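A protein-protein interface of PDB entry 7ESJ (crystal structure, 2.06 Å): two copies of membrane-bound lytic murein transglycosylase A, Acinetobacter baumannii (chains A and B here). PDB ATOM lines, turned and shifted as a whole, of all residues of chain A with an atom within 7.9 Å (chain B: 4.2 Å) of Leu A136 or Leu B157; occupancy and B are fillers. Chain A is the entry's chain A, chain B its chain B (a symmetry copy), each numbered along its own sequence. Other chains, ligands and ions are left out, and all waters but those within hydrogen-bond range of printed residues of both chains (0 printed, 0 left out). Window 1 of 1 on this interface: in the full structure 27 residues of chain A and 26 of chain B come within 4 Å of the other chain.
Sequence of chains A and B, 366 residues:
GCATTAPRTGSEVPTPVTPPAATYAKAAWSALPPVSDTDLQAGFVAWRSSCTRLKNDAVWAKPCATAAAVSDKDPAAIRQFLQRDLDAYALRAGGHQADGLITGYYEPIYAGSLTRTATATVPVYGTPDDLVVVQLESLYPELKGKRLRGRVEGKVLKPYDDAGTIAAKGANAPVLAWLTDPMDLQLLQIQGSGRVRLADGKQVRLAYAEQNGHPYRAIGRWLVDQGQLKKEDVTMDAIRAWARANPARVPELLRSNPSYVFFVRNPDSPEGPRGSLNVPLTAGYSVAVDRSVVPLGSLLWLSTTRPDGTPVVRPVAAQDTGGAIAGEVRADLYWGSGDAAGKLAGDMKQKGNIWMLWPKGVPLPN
Of the 20 printed residues of chain A, 12 touch a printed residue of chain B. Printed residues of chain A that touch a printed residue of chain B: Val A132, Val A133, Val A134, Gln A135, Leu A136, Ser A138, Leu A139, Tyr A140, Val A152, Lys A155, Val A156 and Leu A157. Printed residues of chain B that touch a printed residue of chain A: Val B132, Leu B148, Arg B149, Val B152, Val B156, Leu B157, Lys B158 and Pro B159. Hydrophobic or aromatic side chains of chain B within 4 Å of the printed part of chain A: Val B132, Leu B148, Val B152, Val B156, Leu B157 and Pro B159. Among the printed residues, 19 pairs touch across the chains. Among the printed residues, no Asp or Glu carboxylate lies within 4 Å of a Lys or Arg side-chain nitrogen of the other chain.
O of Gly A150 lies within hydrogen-bond range of N of Val A132. O of Leu A148 sits at hydrogen-bond distance from N of Val A134. O of Gly B150 lies within hydrogen-bond range of N of Val B132 (2.8 Å). N of Val B134 is in hydrogen-bond range of O of Leu B148, 3.1 Å away. N of Lys B158 sits at hydrogen-bond distance from O of Arg B151, 2.9 Å away.
Val A132 touches Leu B157 (CG1 to N, 3.6 Å). Val B156 touches Val A133 (CA to O, 3.3 Å). Leu B157 touches Val A134. O of Gln A135 touches CD of Pro B159 (3.4 Å). Leu B148 touches Leu A136 (CG to CD1, 3.9 Å). Leu A136 touches Pro B159. CG of Pro B159 touches OG of Ser A138 (3.6 Å). CD2 of Leu A139 touches CB of Pro B159, 3.9 Å away. CA of Val B132 touches O of Lys A155, 3.6 Å away. Val B132 touches Val A156.
Leu A136 touches just these residues of chain B: Leu B148 (3.9 Å), Arg B149 (3.5 Å), Leu B157 (3.7 Å), Lys B158 (3.9 Å) and Pro B159 (3.6 Å). Of chain A, only Val A132, Val A133, Val A134, Gln A135 and Leu A136 come within 4 Å of Leu B157. Of the printed residues of chain B, Val A133 touches Val B156 and Leu B157. Of the printed residues of chain B, Leu A157 touches Val B132 (3.6 Å). Of the printed residues of chain A, Arg B149 touches Leu A136. Of the printed residues of chain B, Gln A135 touches Val B156 (3.3 Å), Leu B157 (3.0 Å) and Pro B159 (3.4 Å). Leu A131 touches none of the printed residues of chain B. Gly B150 touches none of the printed residues of chain A. The nearest printed residue of chain B that does not touch Leu A136 is Val B134 (4.2 Å).
Val A132 touches Leu B157, and with the chains exchanged Leu A157 touches Val B132. Val A134 touches Leu B157, but with the chains exchanged Leu A157 does not touch Val B134 (4.01 Å). Val A152 touches its own counterpart, Val B152. Val A156 touches Val B132, but with the chains exchanged Val A132 does not touch Val B156 (4.02 Å). 7 positions are printed for both chains. Of the 19 pairs that touch across the chains among the printed residues, 3 have their exchanged pair printed and touching as well.
The backbone carbonyl oxygen of Val A133 lies within hydrogen-bond range of the backbone NH of Leu B157 (2.9 Å). The backbone NH of Gln A135 lies within hydrogen-bond range of the backbone carbonyl oxygen of Leu B157 (3.0 Å).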
ATOM      1  N   LEU A 131     -32.002 -13.959   0.914  1.00  0.00           N
ATOM      2  CA  LEU A 131     -30.927 -14.895   0.627  1.00  0.00           C
ATOM      3  C   LEU A 131     -29.608 -14.128   0.578  1.00  0.00           C
ATOM      4  O   LEU A 131     -29.434 -13.251  -0.281  1.00  0.00           O
ATOM      5  CB  LEU A 131     -31.188 -15.618  -0.696  1.00  0.00           C
ATOM      6  CG  LEU A 131     -30.140 -16.702  -0.992  1.00  0.00           C
ATOM      7  CD1 LEU A 131     -30.164 -17.767   0.093  1.00  0.00           C
ATOM      8  CD2 LEU A 131     -30.381 -17.345  -2.335  1.00  0.00           C
ATOM      9  N   VAL A 132     -28.676 -14.458   1.488  1.00  0.00           N
ATOM     10  CA  VAL A 132     -27.382 -13.773   1.577  1.00  0.00           C
ATOM     11  C   VAL A 132     -26.296 -14.638   0.940  1.00  0.00           C
ATOM     12  O   VAL A 132     -26.152 -15.821   1.273  1.00  0.00           O
ATOM     13  CB  VAL A 132     -27.025 -13.432   3.036  1.00  0.00           C
ATOM     14  CG1 VAL A 132     -25.747 -12.578   3.090  1.00  0.00           C
ATOM     15  CG2 VAL A 132     -28.159 -12.711   3.702  1.00  0.00           C
ATOM     16  N   VAL A 133     -25.529 -14.048   0.025  1.00  0.00           N
ATOM     17  CA  VAL A 133     -24.381 -14.718  -0.591  1.00  0.00           C
ATOM     18  C   VAL A 133     -23.133 -14.456   0.248  1.00  0.00           C
ATOM     19  O   VAL A 133     -22.735 -13.302   0.449  1.00  0.00           O
ATOM     20  CB  VAL A 133     -24.163 -14.241  -2.034  1.00  0.00           C
ATOM     21  CG1 VAL A 133     -22.833 -14.725  -2.536  1.00  0.00           C
ATOM     22  CG2 VAL A 133     -25.281 -14.740  -2.943  1.00  0.00           C
ATOM     23  N   VAL A 134     -22.492 -15.524   0.708  1.00  0.00           N
ATOM     24  CA  VAL A 134     -21.275 -15.395   1.502  1.00  0.00           C
ATOM     25  C   VAL A 134     -20.086 -15.263   0.567  1.00  0.00           C
ATOM     26  O   VAL A 134     -19.908 -16.064  -0.352  1.00  0.00           O
ATOM     27  CB  VAL A 134     -21.105 -16.593   2.441  1.00  0.00           C
ATOM     28  CG1 VAL A 134     -19.706 -16.596   3.055  1.00  0.00           C
ATOM     29  CG2 VAL A 134     -22.178 -16.555   3.508  1.00  0.00           C
ATOM     30  N   GLN A 135     -19.251 -14.265   0.815  1.00  0.00           N
ATOM     31  CA  GLN A 135     -18.209 -13.871  -0.111  1.00  0.00           C
ATOM     32  C   GLN A 135     -16.971 -13.579   0.735  1.00  0.00           C
ATOM     33  O   GLN A 135     -16.538 -12.438   0.891  1.00  0.00           O
ATOM     34  CB  GLN A 135     -18.674 -12.674  -0.944  1.00  0.00           C
ATOM     35  CG  GLN A 135     -17.751 -12.148  -2.015  1.00  0.00           C
ATOM     36  CD  GLN A 135     -18.272 -10.823  -2.586  1.00  0.00           C
ATOM     37  OE1 GLN A 135     -19.291 -10.793  -3.283  1.00  0.00           O
ATOM     38  NE2 GLN A 135     -17.581  -9.724  -2.280  1.00  0.00           N
ATOM     39  N   LEU A 136     -16.417 -14.642   1.322  1.00  0.00           N
ATOM     40  CA  LEU A 136     -15.271 -14.563   2.212  1.00  0.00           C
ATOM     41  C   LEU A 136     -14.041 -15.203   1.594  1.00  0.00           C
ATOM     42  O   LEU A 136     -13.134 -15.636   2.315  1.00  0.00           O
ATOM     43  CB  LEU A 136     -15.592 -15.228   3.550  1.00  0.00           C
ATOM     44  CG  LEU A 136     -16.637 -14.457   4.363  1.00  0.00           C
ATOM     45  CD1 LEU A 136     -16.913 -15.156   5.681  1.00  0.00           C
ATOM     46  CD2 LEU A 136     -16.164 -13.012   4.598  1.00  0.00           C
ATOM     47  N   GLU A 137     -13.987 -15.270   0.271  1.00  0.00           N
ATOM     48  CA  GLU A 137     -12.928 -16.042  -0.356  1.00  0.00           C
ATOM     49  C   GLU A 137     -11.604 -15.288  -0.363  1.00  0.00           C
ATOM     50  O   GLU A 137     -10.542 -15.920  -0.320  1.00  0.00           O
ATOM     51  CB  GLU A 137     -13.382 -16.469  -1.755  1.00  0.00           C
ATOM     52  CG  GLU A 137     -14.593 -17.395  -1.643  1.00  0.00           C
ATOM     53  CD  GLU A 137     -15.172 -17.842  -2.974  1.00  0.00           C
ATOM     54  OE1 GLU A 137     -14.558 -17.554  -4.028  1.00  0.00           O
ATOM     55  OE2 GLU A 137     -16.246 -18.499  -2.953  1.00  0.00           O
ATOM     56  N   SER A 138     -11.639 -13.951  -0.354  1.00  0.00           N
ATOM     57  CA  SER A 138     -10.393 -13.194  -0.224  1.00  0.00           C
ATOM     58  C   SER A 138      -9.663 -13.530   1.073  1.00  0.00           C
ATOM     59  O   SER A 138      -8.432 -13.437   1.130  1.00  0.00           O
ATOM     60  CB  SER A 138     -10.666 -11.691  -0.307  1.00  0.00           C
ATOM     61  OG  SER A 138     -11.628 -11.280   0.648  1.00  0.00           O
ATOM     62  N   LEU A 139     -10.398 -13.935   2.110  1.00  0.00           N
ATOM     63  CA  LEU A 139      -9.816 -14.320   3.391  1.00  0.00           C
ATOM     64  C   LEU A 139      -9.487 -15.801   3.460  1.00  0.00           C
ATOM     65  O   LEU A 139      -8.519 -16.187   4.124  1.00  0.00           O
ATOM     66  CB  LEU A 139     -10.778 -13.966   4.536  1.00  0.00           C
ATOM     67  CG  LEU A 139     -10.731 -12.572   5.172  1.00  0.00           C
ATOM     68  CD1 LEU A 139     -10.561 -11.469   4.145  1.00  0.00           C
ATOM     69  CD2 LEU A 139     -11.977 -12.316   5.984  1.00  0.00           C
ATOM     70  N   TYR A 140     -10.280 -16.648   2.812  1.00  0.00           N
ATOM     71  CA  TYR A 140     -10.069 -18.092   2.829  1.00  0.00           C
ATOM     72  C   TYR A 140     -10.198 -18.586   1.400  1.00  0.00           C
ATOM     73  O   TYR A 140     -11.279 -19.016   0.980  1.00  0.00           O
ATOM     74  CB  TYR A 140     -11.057 -18.792   3.757  1.00  0.00           C
ATOM     75  CG  TYR A 140     -10.992 -18.254   5.156  1.00  0.00           C
ATOM     76  CD1 TYR A 140     -11.751 -17.148   5.515  1.00  0.00           C
ATOM     77  CD2 TYR A 140     -10.161 -18.830   6.114  1.00  0.00           C
ATOM     78  CE1 TYR A 140     -11.696 -16.624   6.777  1.00  0.00           C
ATOM     79  CE2 TYR A 140     -10.099 -18.313   7.394  1.00  0.00           C
ATOM     80  CZ  TYR A 140     -10.876 -17.204   7.719  1.00  0.00           C
ATOM     81  OH  TYR A 140     -10.852 -16.641   8.973  1.00  0.00           O
ATOM     82  N   PRO A 141      -9.111 -18.545   0.624  1.00  0.00           N
ATOM     83  CA  PRO A 141      -9.206 -18.932  -0.796  1.00  0.00           C
ATOM     84  C   PRO A 141      -9.698 -20.362  -1.017  1.00  0.00           C
ATOM     85  O   PRO A 141     -10.107 -20.695  -2.136  1.00  0.00           O
ATOM     86  CB  PRO A 141      -7.771 -18.728  -1.315  1.00  0.00           C
ATOM     87  CG  PRO A 141      -6.911 -18.720  -0.078  1.00  0.00           C
ATOM     88  CD  PRO A 141      -7.753 -18.122   1.001  1.00  0.00           C
ATOM     89  N   GLU A 142      -9.704 -21.207   0.018  1.00  0.00           N
ATOM     90  CA  GLU A 142     -10.193 -22.574  -0.123  1.00  0.00           C
ATOM     91  C   GLU A 142     -11.708 -22.659  -0.265  1.00  0.00           C
ATOM     92  O   GLU A 142     -12.222 -23.734  -0.600  1.00  0.00           O
ATOM     93  CB  GLU A 142      -9.742 -23.416   1.069  1.00  0.00           C
ATOM     94  CG  GLU A 142     -10.286 -22.962   2.407  1.00  0.00           C
ATOM     95  CD  GLU A 142      -9.371 -21.958   3.096  1.00  0.00           C
ATOM     96  OE1 GLU A 142      -8.844 -21.057   2.403  1.00  0.00           O
ATOM     97  OE2 GLU A 142      -9.171 -22.079   4.326  1.00  0.00           O
ATOM     98  N   LEU A 143     -12.431 -21.571  -0.008  1.00  0.00           N
ATOM     99  CA  LEU A 143     -13.869 -21.526  -0.223  1.00  0.00           C
ATOM    100  C   LEU A 143     -14.245 -21.346  -1.685  1.00  0.00           C
ATOM    101  O   LEU A 143     -15.439 -21.381  -1.999  1.00  0.00           O
ATOM    102  CB  LEU A 143     -14.485 -20.380   0.589  1.00  0.00           C
ATOM    103  CG  LEU A 143     -14.219 -20.408   2.086  1.00  0.00           C
ATOM    104  CD1 LEU A 143     -14.841 -19.191   2.756  1.00  0.00           C
ATOM    105  CD2 LEU A 143     -14.759 -21.693   2.663  1.00  0.00           C
ATOM    106  N   LYS A 144     -13.268 -21.164  -2.580  1.00  0.00           N
ATOM    107  CA  LYS A 144     -13.554 -20.618  -3.907  1.00  0.00           C
ATOM    108  C   LYS A 144     -14.450 -21.514  -4.751  1.00  0.00           C
ATOM    109  O   LYS A 144     -15.148 -21.007  -5.641  1.00  0.00           O
ATOM    110  CB  LYS A 144     -12.255 -20.334  -4.663  1.00  0.00           C
ATOM    111  CG  LYS A 144     -12.437 -19.415  -5.868  1.00  0.00           C
ATOM    112  CD  LYS A 144     -11.488 -19.780  -7.010  1.00  0.00           C
ATOM    113  CE  LYS A 144     -10.100 -20.128  -6.485  1.00  0.00           C
ATOM    114  NZ  LYS A 144      -9.027 -19.875  -7.489  1.00  0.00           N
ATOM    115  N   LEU A 148     -21.639 -20.772  -0.889  1.00  0.00           N
ATOM    116  CA  LEU A 148     -22.091 -20.629   0.483  1.00  0.00           C
ATOM    117  C   LEU A 148     -23.178 -19.567   0.516  1.00  0.00           C
ATOM    118  O   LEU A 148     -23.005 -18.477  -0.041  1.00  0.00           O
ATOM    119  CB  LEU A 148     -20.942 -20.254   1.409  1.00  0.00           C
ATOM    120  CG  LEU A 148     -19.810 -21.273   1.447  1.00  0.00           C
ATOM    121  CD1 LEU A 148     -18.610 -20.651   2.125  1.00  0.00           C
ATOM    122  CD2 LEU A 148     -20.261 -22.525   2.170  1.00  0.00           C
ATOM    123  N   GLY A 150     -26.839 -18.199   2.989  1.00  0.00           N
ATOM    124  CA  GLY A 150     -27.579 -18.370   4.217  1.00  0.00           C
ATOM    125  C   GLY A 150     -28.637 -17.311   4.388  1.00  0.00           C
ATOM    126  O   GLY A 150     -28.879 -16.482   3.502  1.00  0.00           O
ATOM    127  N   VAL A 152     -29.846 -14.471   7.497  1.00  0.00           N
ATOM    128  CA  VAL A 152     -29.352 -13.815   8.701  1.00  0.00           C
ATOM    129  C   VAL A 152     -30.441 -13.839   9.760  1.00  0.00           C
ATOM    130  O   VAL A 152     -31.539 -13.318   9.553  1.00  0.00           O
ATOM    131  CB  VAL A 152     -28.892 -12.381   8.415  1.00  0.00           C
ATOM    132  CG1 VAL A 152     -28.751 -11.612   9.725  1.00  0.00           C
ATOM    133  CG2 VAL A 152     -27.578 -12.413   7.650  1.00  0.00           C
ATOM    134  N   LYS A 155     -27.656 -12.065  14.855  1.00  0.00           N
ATOM    135  CA  LYS A 155     -26.283 -11.827  14.435  1.00  0.00           C
ATOM    136  C   LYS A 155     -25.632 -13.085  13.873  1.00  0.00           C
ATOM    137  O   LYS A 155     -24.408 -13.226  13.927  1.00  0.00           O
ATOM    138  CB  LYS A 155     -25.461 -11.280  15.602  1.00  0.00           C
ATOM    139  CG  LYS A 155     -26.122 -10.122  16.334  1.00  0.00           C
ATOM    140  CD  LYS A 155     -25.294  -9.635  17.536  1.00  0.00           C
ATOM    141  CE  LYS A 155     -23.837  -9.390  17.130  1.00  0.00           C
ATOM    142  NZ  LYS A 155     -23.039  -8.765  18.216  1.00  0.00           N
ATOM    143  N   VAL A 156     -26.431 -14.001  13.329  1.00  0.00           N
ATOM    144  CA  VAL A 156     -25.961 -15.283  12.821  1.00  0.00           C
ATOM    145  C   VAL A 156     -26.452 -15.477  11.392  1.00  0.00           C
ATOM    146  O   VAL A 156     -27.626 -15.238  11.097  1.00  0.00           O
ATOM    147  CB  VAL A 156     -26.458 -16.449  13.698  1.00  0.00           C
ATOM    148  CG1 VAL A 156     -25.739 -17.723  13.305  1.00  0.00           C
ATOM    149  CG2 VAL A 156     -26.281 -16.121  15.184  1.00  0.00           C
ATOM    150  N   LEU A 157     -25.551 -15.915  10.507  1.00  0.00           N
ATOM    151  CA  LEU A 157     -25.929 -16.412   9.183  1.00  0.00           C
ATOM    152  C   LEU A 157     -26.148 -17.918   9.290  1.00  0.00           C
ATOM    153  O   LEU A 157     -25.189 -18.696   9.387  1.00  0.00           O
ATOM    154  CB  LEU A 157     -24.870 -16.085   8.134  1.00  0.00           C
ATOM    155  CG  LEU A 157     -25.323 -16.574   6.741  1.00  0.00           C
ATOM    156  CD1 LEU A 157     -25.470 -15.450   5.727  1.00  0.00           C
ATOM    157  CD2 LEU A 157     -24.387 -17.638   6.208  1.00  0.00           C
ATOM    158  N   VAL B 132     -21.548 -10.367  11.732  1.00  0.00           N
ATOM    159  CA  VAL B 132     -22.358 -11.562  11.520  1.00  0.00           C
ATOM    160  C   VAL B 132     -21.450 -12.786  11.594  1.00  0.00           C
ATOM    161  O   VAL B 132     -20.454 -12.883  10.869  1.00  0.00           O
ATOM    162  CB  VAL B 132     -23.114 -11.497  10.185  1.00  0.00           C
ATOM    163  CG1 VAL B 132     -24.016 -12.737  10.001  1.00  0.00           C
ATOM    164  CG2 VAL B 132     -23.954 -10.216  10.127  1.00  0.00           C
ATOM    165  N   VAL B 134     -20.867 -16.393  10.615  1.00  0.00           N
ATOM    166  CA  VAL B 134     -21.278 -17.409   9.653  1.00  0.00           C
ATOM    167  C   VAL B 134     -21.292 -18.768  10.340  1.00  0.00           C
ATOM    168  O   VAL B 134     -20.340 -19.132  11.042  1.00  0.00           O
ATOM    169  CB  VAL B 134     -20.334 -17.420   8.440  1.00  0.00           C
ATOM    170  CG1 VAL B 134     -20.629 -18.634   7.540  1.00  0.00           C
ATOM    171  CG2 VAL B 134     -20.460 -16.117   7.659  1.00  0.00           C
ATOM    172  N   LEU B 148     -15.516 -17.807  10.644  1.00  0.00           N
ATOM    173  CA  LEU B 148     -15.969 -17.023   9.508  1.00  0.00           C
ATOM    174  C   LEU B 148     -16.897 -15.940  10.022  1.00  0.00           C
ATOM    175  O   LEU B 148     -17.798 -16.227  10.817  1.00  0.00           O
ATOM    176  CB  LEU B 148     -16.690 -17.910   8.494  1.00  0.00           C
ATOM    177  CG  LEU B 148     -15.837 -18.494   7.373  1.00  0.00           C
ATOM    178  CD1 LEU B 148     -14.511 -19.012   7.876  1.00  0.00           C
ATOM    179  CD2 LEU B 148     -16.621 -19.602   6.695  1.00  0.00           C
ATOM    180  N   ARG B 149     -16.646 -14.696   9.605  1.00  0.00           N
ATOM    181  CA  ARG B 149     -17.449 -13.568  10.044  1.00  0.00           C
ATOM    182  C   ARG B 149     -17.494 -12.541   8.927  1.00  0.00           C
ATOM    183  O   ARG B 149     -16.620 -12.497   8.059  1.00  0.00           O
ATOM    184  CB  ARG B 149     -16.901 -12.904  11.316  1.00  0.00           C
ATOM    185  CG  ARG B 149     -17.312 -13.583  12.609  1.00  0.00           C
ATOM    186  CD  ARG B 149     -16.142 -14.389  13.115  1.00  0.00           C
ATOM    187  NE  ARG B 149     -16.406 -15.036  14.398  1.00  0.00           N
ATOM    188  CZ  ARG B 149     -16.831 -16.293  14.524  1.00  0.00           C
ATOM    189  NH1 ARG B 149     -17.070 -17.031  13.445  1.00  0.00           N
ATOM    190  NH2 ARG B 149     -17.030 -16.814  15.725  1.00  0.00           N
ATOM    191  N   GLY B 150     -18.512 -11.696   8.979  1.00  0.00           N
ATOM    192  CA  GLY B 150     -18.561 -10.639   7.994  1.00  0.00           C
ATOM    193  C   GLY B 150     -19.584  -9.596   8.359  1.00  0.00           C
ATOM    194  O   GLY B 150     -20.224  -9.642   9.417  1.00  0.00           O
ATOM    195  N   ARG B 151     -19.704  -8.641   7.454  1.00  0.00           N
ATOM    196  CA  ARG B 151     -20.707  -7.594   7.497  1.00  0.00           C
ATOM    197  C   ARG B 151     -21.620  -7.781   6.295  1.00  0.00           C
ATOM    198  O   ARG B 151     -21.152  -8.064   5.185  1.00  0.00           O
ATOM    199  CB  ARG B 151     -20.051  -6.199   7.455  1.00  0.00           C
ATOM    200  CG  ARG B 151     -21.058  -5.053   7.412  1.00  0.00           C
ATOM    201  CD  ARG B 151     -20.372  -3.708   7.234  1.00  0.00           C
ATOM    202  NE  ARG B 151     -19.948  -3.133   8.510  1.00  0.00           N
ATOM    203  CZ  ARG B 151     -18.679  -2.962   8.871  1.00  0.00           C
ATOM    204  NH1 ARG B 151     -17.690  -3.345   8.067  1.00  0.00           N
ATOM    205  NH2 ARG B 151     -18.397  -2.434  10.048  1.00  0.00           N
ATOM    206  N   VAL B 152     -22.913  -7.641   6.501  1.00  0.00           N
ATOM    207  CA  VAL B 152     -23.860  -7.853   5.419  1.00  0.00           C
ATOM    208  C   VAL B 152     -24.144  -6.502   4.784  1.00  0.00           C
ATOM    209  O   VAL B 152     -24.691  -5.608   5.434  1.00  0.00           O
ATOM    210  CB  VAL B 152     -25.150  -8.523   5.914  1.00  0.00           C
ATOM    211  CG1 VAL B 152     -26.179  -8.542   4.796  1.00  0.00           C
ATOM    212  CG2 VAL B 152     -24.853  -9.953   6.397  1.00  0.00           C
ATOM    213  N   VAL B 156     -24.958  -9.448   0.329  1.00  0.00           N
ATOM    214  CA  VAL B 156     -23.648 -10.087   0.353  1.00  0.00           C
ATOM    215  C   VAL B 156     -23.035  -9.941   1.738  1.00  0.00           C
ATOM    216  O   VAL B 156     -22.971  -8.835   2.285  1.00  0.00           O
ATOM    217  CB  VAL B 156     -22.700  -9.503  -0.704  1.00  0.00           C
ATOM    218  CG1 VAL B 156     -21.486 -10.378  -0.811  1.00  0.00           C
ATOM    219  CG2 VAL B 156     -23.387  -9.404  -2.047  1.00  0.00           C
ATOM    220  N   LEU B 157     -22.583 -11.058   2.297  1.00  0.00           N
ATOM    221  CA  LEU B 157     -21.747 -11.047   3.486  1.00  0.00           C
ATOM    222  C   LEU B 157     -20.309 -10.880   3.011  1.00  0.00           C
ATOM    223  O   LEU B 157     -19.768 -11.755   2.328  1.00  0.00           O
ATOM    224  CB  LEU B 157     -21.930 -12.322   4.305  1.00  0.00           C
ATOM    225  CG  LEU B 157     -21.302 -12.293   5.705  1.00  0.00           C
ATOM    226  CD1 LEU B 157     -22.262 -12.882   6.723  1.00  0.00           C
ATOM    227  CD2 LEU B 157     -19.979 -13.052   5.724  1.00  0.00           C
ATOM    228  N   LYS B 158     -19.708  -9.743   3.339  1.00  0.00           N
ATOM    229  CA  LYS B 158     -18.365  -9.383   2.916  1.00  0.00           C
ATOM    230  C   LYS B 158     -17.434  -9.382   4.121  1.00  0.00           C
ATOM    231  O   LYS B 158     -17.898  -9.329   5.266  1.00  0.00           O
ATOM    232  CB  LYS B 158     -18.376  -8.002   2.238  1.00  0.00           C
ATOM    233  CG  LYS B 158     -19.219  -7.947   0.946  1.00  0.00           C
ATOM    234  CD  LYS B 158     -19.318  -6.530   0.384  1.00  0.00           C
ATOM    235  CE  LYS B 158     -17.987  -6.085  -0.226  1.00  0.00           C
ATOM    236  NZ  LYS B 158     -17.964  -4.650  -0.650  1.00  0.00           N
ATOM    237  N   PRO B 159     -16.120  -9.495   3.903  1.00  0.00           N
ATOM    238  CA  PRO B 159     -15.169  -9.442   5.026  1.00  0.00           C
ATOM    239  C   PRO B 159     -15.459  -8.274   5.962  1.00  0.00           C
ATOM    240  O   PRO B 159     -15.833  -7.186   5.521  1.00  0.00           O
ATOM    241  CB  PRO B 159     -13.815  -9.267   4.329  1.00  0.00           C
ATOM    242  CG  PRO B 159     -14.017  -9.847   2.927  1.00  0.00           C
ATOM    243  CD  PRO B 159     -15.451  -9.662   2.590  1.00  0.00           C
